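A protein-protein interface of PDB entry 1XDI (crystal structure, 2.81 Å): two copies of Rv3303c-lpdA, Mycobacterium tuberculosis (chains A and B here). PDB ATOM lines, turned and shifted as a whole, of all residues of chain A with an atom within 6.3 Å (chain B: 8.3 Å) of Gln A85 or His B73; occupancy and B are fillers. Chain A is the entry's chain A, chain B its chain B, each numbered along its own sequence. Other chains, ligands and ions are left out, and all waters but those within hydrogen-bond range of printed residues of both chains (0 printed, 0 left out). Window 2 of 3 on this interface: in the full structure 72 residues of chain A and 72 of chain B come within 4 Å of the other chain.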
ATOM      1  N   LYS A  80      29.767  -8.991  12.890  1.00  0.00           N
ATOM      2  CA  LYS A  80      30.641 -10.147  12.734  1.00  0.00           C
ATOM      3  C   LYS A  80      29.951 -11.527  12.875  1.00  0.00           C
ATOM      4  O   LYS A  80      29.208 -11.781  13.814  1.00  0.00           O
ATOM      5  CB  LYS A  80      31.750 -10.129  13.778  1.00  0.00           C
ATOM      6  CG  LYS A  80      32.846  -9.086  13.675  1.00  0.00           C
ATOM      7  CD  LYS A  80      33.935  -9.438  14.758  1.00  0.00           C
ATOM      8  CE  LYS A  80      35.271  -8.651  14.647  1.00  0.00           C
ATOM      9  NZ  LYS A  80      36.411  -9.418  15.279  1.00  0.00           N
ATOM     10  N   ILE A  81      30.247 -12.428  11.945  1.00  0.00           N
ATOM     11  CA  ILE A  81      29.743 -13.799  11.941  1.00  0.00           C
ATOM     12  C   ILE A  81      31.000 -14.594  12.206  1.00  0.00           C
ATOM     13  O   ILE A  81      31.956 -14.469  11.476  1.00  0.00           O
ATOM     14  CB  ILE A  81      29.229 -14.187  10.570  1.00  0.00           C
ATOM     15  CG1 ILE A  81      27.782 -13.752  10.420  1.00  0.00           C
ATOM     16  CG2 ILE A  81      29.359 -15.661  10.367  1.00  0.00           C
ATOM     17  CD1 ILE A  81      27.258 -13.853   8.968  1.00  0.00           C
ATOM     18  N   SER A  82      31.018 -15.407  13.246  1.00  0.00           N
ATOM     19  CA  SER A  82      32.217 -16.186  13.570  1.00  0.00           C
ATOM     20  C   SER A  82      32.189 -17.655  13.216  1.00  0.00           C
ATOM     21  O   SER A  82      32.029 -18.487  14.100  1.00  0.00           O
ATOM     22  CB  SER A  82      32.506 -16.101  15.052  1.00  0.00           C
ATOM     23  OG  SER A  82      33.490 -17.063  15.336  1.00  0.00           O
ATOM     24  N   LEU A  83      32.383 -17.994  11.955  1.00  0.00           N
ATOM     25  CA  LEU A  83      32.323 -19.398  11.537  1.00  0.00           C
ATOM     26  C   LEU A  83      33.001 -20.415  12.477  1.00  0.00           C
ATOM     27  O   LEU A  83      32.426 -21.449  12.773  1.00  0.00           O
ATOM     28  CB  LEU A  83      32.862 -19.540  10.093  1.00  0.00           C
ATOM     29  CG  LEU A  83      32.108 -20.359   9.036  1.00  0.00           C
ATOM     30  CD1 LEU A  83      32.976 -21.491   8.739  1.00  0.00           C
ATOM     31  CD2 LEU A  83      30.726 -20.860   9.471  1.00  0.00           C
ATOM     32  N   PRO A  84      34.203 -20.118  12.985  1.00  0.00           N
ATOM     33  CA  PRO A  84      34.831 -21.091  13.865  1.00  0.00           C
ATOM     34  C   PRO A  84      34.033 -21.445  15.103  1.00  0.00           C
ATOM     35  O   PRO A  84      34.052 -22.611  15.526  1.00  0.00           O
ATOM     36  CB  PRO A  84      36.161 -20.450  14.205  1.00  0.00           C
ATOM     37  CG  PRO A  84      36.455 -19.646  13.039  1.00  0.00           C
ATOM     38  CD  PRO A  84      35.116 -18.997  12.761  1.00  0.00           C
ATOM     39  N   GLN A  85      33.357 -20.484  15.724  1.00  0.00           N
ATOM     40  CA  GLN A  85      32.587 -20.893  16.888  1.00  0.00           C
ATOM     41  C   GLN A  85      31.306 -21.656  16.474  1.00  0.00           C
ATOM     42  O   GLN A  85      30.834 -22.524  17.232  1.00  0.00           O
ATOM     43  CB  GLN A  85      32.305 -19.740  17.874  1.00  0.00           C
ATOM     44  CG  GLN A  85      32.075 -18.409  17.290  1.00  0.00           C
ATOM     45  CD  GLN A  85      32.080 -17.298  18.360  1.00  0.00           C
ATOM     46  OE1 GLN A  85      31.141 -17.182  19.157  1.00  0.00           O
ATOM     47  NE2 GLN A  85      33.144 -16.478  18.373  1.00  0.00           N
ATOM     48  N   ILE A  86      30.766 -21.384  15.281  1.00  0.00           N
ATOM     49  CA  ILE A  86      29.601 -22.135  14.825  1.00  0.00           C
ATOM     50  C   ILE A  86      30.064 -23.607  14.693  1.00  0.00           C
ATOM     51  O   ILE A  86      29.426 -24.529  15.247  1.00  0.00           O
ATOM     52  CB  ILE A  86      29.099 -21.650  13.441  1.00  0.00           C
ATOM     53  CG1 ILE A  86      28.330 -20.360  13.580  1.00  0.00           C
ATOM     54  CG2 ILE A  86      28.204 -22.701  12.784  1.00  0.00           C
ATOM     55  CD1 ILE A  86      28.202 -19.656  12.259  1.00  0.00           C
ATOM     56  N   HIS A  87      31.160 -23.817  13.955  1.00  0.00           N
ATOM     57  CA  HIS A  87      31.743 -25.150  13.738  1.00  0.00           C
ATOM     58  C   HIS A  87      32.028 -25.819  15.115  1.00  0.00           C
ATOM     59  O   HIS A  87      31.726 -26.975  15.351  1.00  0.00           O
ATOM     60  CB  HIS A  87      33.046 -25.014  12.927  1.00  0.00           C
ATOM     61  CG  HIS A  87      32.846 -24.666  11.481  1.00  0.00           C
ATOM     62  ND1 HIS A  87      33.898 -24.541  10.597  1.00  0.00           N
ATOM     63  CD2 HIS A  87      31.719 -24.538  10.733  1.00  0.00           C
ATOM     64  CE1 HIS A  87      33.428 -24.368   9.374  1.00  0.00           C
ATOM     65  NE2 HIS A  87      32.109 -24.363   9.425  1.00  0.00           N
ATOM     66  N   ALA A  88      32.604 -25.066  16.041  1.00  0.00           N
ATOM     67  CA  ALA A  88      32.936 -25.601  17.355  1.00  0.00           C
ATOM     68  C   ALA A  88      31.655 -26.099  18.055  1.00  0.00           C
ATOM     69  O   ALA A  88      31.668 -27.065  18.867  1.00  0.00           O
ATOM     70  CB  ALA A  88      33.618 -24.542  18.160  1.00  0.00           C
ATOM     71  N   ARG A  89      30.544 -25.433  17.737  1.00  0.00           N
ATOM     72  CA  ARG A  89      29.280 -25.796  18.343  1.00  0.00           C
ATOM     73  C   ARG A  89      28.808 -27.000  17.607  1.00  0.00           C
ATOM     74  O   ARG A  89      28.102 -27.848  18.163  1.00  0.00           O
ATOM     75  CB  ARG A  89      28.255 -24.718  18.200  1.00  0.00           C
ATOM     76  CG  ARG A  89      26.990 -25.124  18.795  1.00  0.00           C
ATOM     77  CD  ARG A  89      25.831 -24.303  18.223  1.00  0.00           C
ATOM     78  NE  ARG A  89      24.597 -24.574  18.953  1.00  0.00           N
ATOM     79  CZ  ARG A  89      23.372 -24.417  18.470  1.00  0.00           C
ATOM     80  NH1 ARG A  89      23.168 -23.975  17.224  1.00  0.00           N
ATOM     81  NH2 ARG A  89      22.341 -24.718  19.256  1.00  0.00           N
ATOM     82  N   VAL A  90      29.211 -27.101  16.347  1.00  0.00           N
ATOM     83  CA  VAL A  90      28.791 -28.250  15.587  1.00  0.00           C
ATOM     84  C   VAL A  90      29.467 -29.494  16.104  1.00  0.00           C
ATOM     85  O   VAL A  90      28.796 -30.496  16.302  1.00  0.00           O
ATOM     86  CB  VAL A  90      29.055 -28.048  14.099  1.00  0.00           C
ATOM     87  CG1 VAL A  90      28.965 -29.376  13.306  1.00  0.00           C
ATOM     88  CG2 VAL A  90      28.052 -27.073  13.616  1.00  0.00           C
ATOM     89  N   LEU B  64      18.446 -12.176  20.978  1.00  0.00           N
ATOM     90  CA  LEU B  64      19.493 -11.216  20.657  1.00  0.00           C
ATOM     91  C   LEU B  64      20.577 -11.375  21.722  1.00  0.00           C
ATOM     92  O   LEU B  64      21.736 -11.607  21.414  1.00  0.00           O
ATOM     93  CB  LEU B  64      18.951  -9.786  20.684  1.00  0.00           C
ATOM     94  CG  LEU B  64      18.383  -9.163  19.402  1.00  0.00           C
ATOM     95  CD1 LEU B  64      17.216  -8.245  19.744  1.00  0.00           C
ATOM     96  CD2 LEU B  64      19.464  -8.396  18.687  1.00  0.00           C
ATOM     97  N   ALA B  67      22.757 -14.228  20.815  1.00  0.00           N
ATOM     98  CA  ALA B  67      23.546 -14.405  19.601  1.00  0.00           C
ATOM     99  C   ALA B  67      25.076 -14.517  19.720  1.00  0.00           C
ATOM    100  O   ALA B  67      25.687 -15.332  19.039  1.00  0.00           O
ATOM    101  CB  ALA B  67      23.198 -13.320  18.624  1.00  0.00           C
ATOM    102  N   PRO B  68      25.718 -13.701  20.574  1.00  0.00           N
ATOM    103  CA  PRO B  68      27.177 -13.790  20.688  1.00  0.00           C
ATOM    104  C   PRO B  68      27.750 -15.175  20.868  1.00  0.00           C
ATOM    105  O   PRO B  68      28.753 -15.499  20.240  1.00  0.00           O
ATOM    106  CB  PRO B  68      27.499 -12.882  21.861  1.00  0.00           C
ATOM    107  CG  PRO B  68      26.441 -11.843  21.755  1.00  0.00           C
ATOM    108  CD  PRO B  68      25.192 -12.656  21.473  1.00  0.00           C
ATOM    109  N   HIS B  69      27.158 -16.013  21.708  1.00  0.00           N
ATOM    110  CA  HIS B  69      27.751 -17.332  21.846  1.00  0.00           C
ATOM    111  C   HIS B  69      27.380 -18.218  20.650  1.00  0.00           C
ATOM    112  O   HIS B  69      28.056 -19.203  20.321  1.00  0.00           O
ATOM    113  CB  HIS B  69      27.383 -17.957  23.197  1.00  0.00           C
ATOM    114  CG  HIS B  69      25.988 -18.514  23.285  1.00  0.00           C
ATOM    115  ND1 HIS B  69      24.854 -17.725  23.246  1.00  0.00           N
ATOM    116  CD2 HIS B  69      25.551 -19.781  23.498  1.00  0.00           C
ATOM    117  CE1 HIS B  69      23.787 -18.482  23.434  1.00  0.00           C
ATOM    118  NE2 HIS B  69      24.182 -19.732  23.589  1.00  0.00           N
ATOM    119  N   LEU B  70      26.322 -17.831  19.952  1.00  0.00           N
ATOM    120  CA  LEU B  70      25.900 -18.582  18.769  1.00  0.00           C
ATOM    121  C   LEU B  70      26.744 -18.193  17.543  1.00  0.00           C
ATOM    122  O   LEU B  70      26.451 -18.579  16.401  1.00  0.00           O
ATOM    123  CB  LEU B  70      24.401 -18.383  18.525  1.00  0.00           C
ATOM    124  CG  LEU B  70      23.580 -19.308  19.407  1.00  0.00           C
ATOM    125  CD1 LEU B  70      22.132 -18.915  19.377  1.00  0.00           C
ATOM    126  CD2 LEU B  70      23.778 -20.726  18.924  1.00  0.00           C
ATOM    127  N   GLY B  71      27.797 -17.425  17.814  1.00  0.00           N
ATOM    128  CA  GLY B  71      28.720 -17.021  16.775  1.00  0.00           C
ATOM    129  C   GLY B  71      28.531 -15.673  16.120  1.00  0.00           C
ATOM    130  O   GLY B  71      29.361 -15.299  15.296  1.00  0.00           O
ATOM    131  N   PHE B  72      27.475 -14.934  16.459  1.00  0.00           N
ATOM    132  CA  PHE B  72      27.233 -13.625  15.835  1.00  0.00           C
ATOM    133  C   PHE B  72      27.398 -12.453  16.790  1.00  0.00           C
ATOM    134  O   PHE B  72      26.552 -12.188  17.655  1.00  0.00           O
ATOM    135  CB  PHE B  72      25.836 -13.556  15.238  1.00  0.00           C
ATOM    136  CG  PHE B  72      25.492 -14.710  14.374  1.00  0.00           C
ATOM    137  CD1 PHE B  72      25.112 -15.916  14.937  1.00  0.00           C
ATOM    138  CD2 PHE B  72      25.568 -14.604  12.991  1.00  0.00           C
ATOM    139  CE1 PHE B  72      24.816 -17.016  14.120  1.00  0.00           C
ATOM    140  CE2 PHE B  72      25.278 -15.682  12.177  1.00  0.00           C
ATOM    141  CZ  PHE B  72      24.901 -16.897  12.736  1.00  0.00           C
ATOM    142  N   HIS B  73      28.490 -11.728  16.588  1.00  0.00           N
ATOM    143  CA  HIS B  73      28.852 -10.578  17.392  1.00  0.00           C
ATOM    144  C   HIS B  73      28.343  -9.275  16.795  1.00  0.00           C
ATOM    145  O   HIS B  73      27.247  -8.813  17.143  1.00  0.00           O
ATOM    146  CB  HIS B  73      30.355 -10.607  17.510  1.00  0.00           C
ATOM    147  CG  HIS B  73      30.863 -11.947  17.920  1.00  0.00           C
ATOM    148  ND1 HIS B  73      30.667 -12.452  19.185  1.00  0.00           N
ATOM    149  CD2 HIS B  73      31.487 -12.923  17.220  1.00  0.00           C
ATOM    150  CE1 HIS B  73      31.149 -13.681  19.249  1.00  0.00           C
ATOM    151  NE2 HIS B  73      31.652 -13.991  18.068  1.00  0.00           N
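No position is printed for both chains. Of the 13 pairs that touch across the chains among the printed residues, none has its exchanged pair printed and touching as well.
The side-chain hydroxyl (OG) of Ser A82 lies close to the side-chain amide nitrogen (NE2) of Gln A85, at 3.1 Å. O of Ala B67 lies within hydrogen-bond range of N of Phe B72 (3.2 Å).
The backbone carbonyl oxygen (O) of Lys A80 lies within hydrogen-bond range of the backbone NH (N) of His B73, 2.9 Å away. The backbone NH (N) of Ser A82 sits at hydrogen-bond distance from the backbone carbonyl oxygen (O) of Gly B71, at 2.6 Å. O of Pro B68 lies close to OE1 of Gln A85 (3.1 Å). The side-chain amide nitrogen of Gln A85 sits at hydrogen-bond distance from a ring nitrogen (NE2) of His B73.
Hydrophobic or aromatic side chains of chain B within 4 Å of the printed part of chain A: Leu B70, Phe B72 and His B73. Of the 11 printed residues of chain A, 6 touch a printed residue of chain B. Hydrophobic or aromatic side chains of chain A within 4 Å of the printed part of chain B: Ile A81 and Ile A86. Among the printed residues, no Asp or Glu carboxylate lies within 4 Å of a Lys or Arg side-chain nitrogen of the other chain.
Of chain A, only Lys A80, Ser A82 and Gln A85 come within 4 Å of His B73. No residue of chain B comes within 4 Å of Pro A84. Printed residues of chain B within 4 Å of Arg A89: Leu B70. Printed residues of chain B within 4 Å of Ser A82: Gly B71 (2.6 Å) and His B73 (3.8 Å). Of the printed residues of chain A, Gly B71 touches Lys A80, Ile A81, Ser A82 and Gln A85. Of the printed residues of chain A, Pro B68 touches Gln A85 (3.1 Å). Ala B67 touches none of the printed residues of chain A. The nearest residue of chain A that does not touch His B73 is Ile A81 (5.0 Å).
Among the printed residues, pairs that only touch across the chains: Lys A80 with Gly B71 (3.8 Å), Lys A80 with Phe B72 (3.4 Å), Ile A81 with Gly B71 (3.6 Å), Ile A81 with Phe B72 (3.5 Å), Ser A82 with His B73 (3.8 Å), Gln A85 with His B69 (3.9 Å), Gln A85 with Gly B71 (3.4 Å), Ile A86 with Leu B70 (3.8 Å) and Arg A89 with Leu B70 (3.7 Å).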
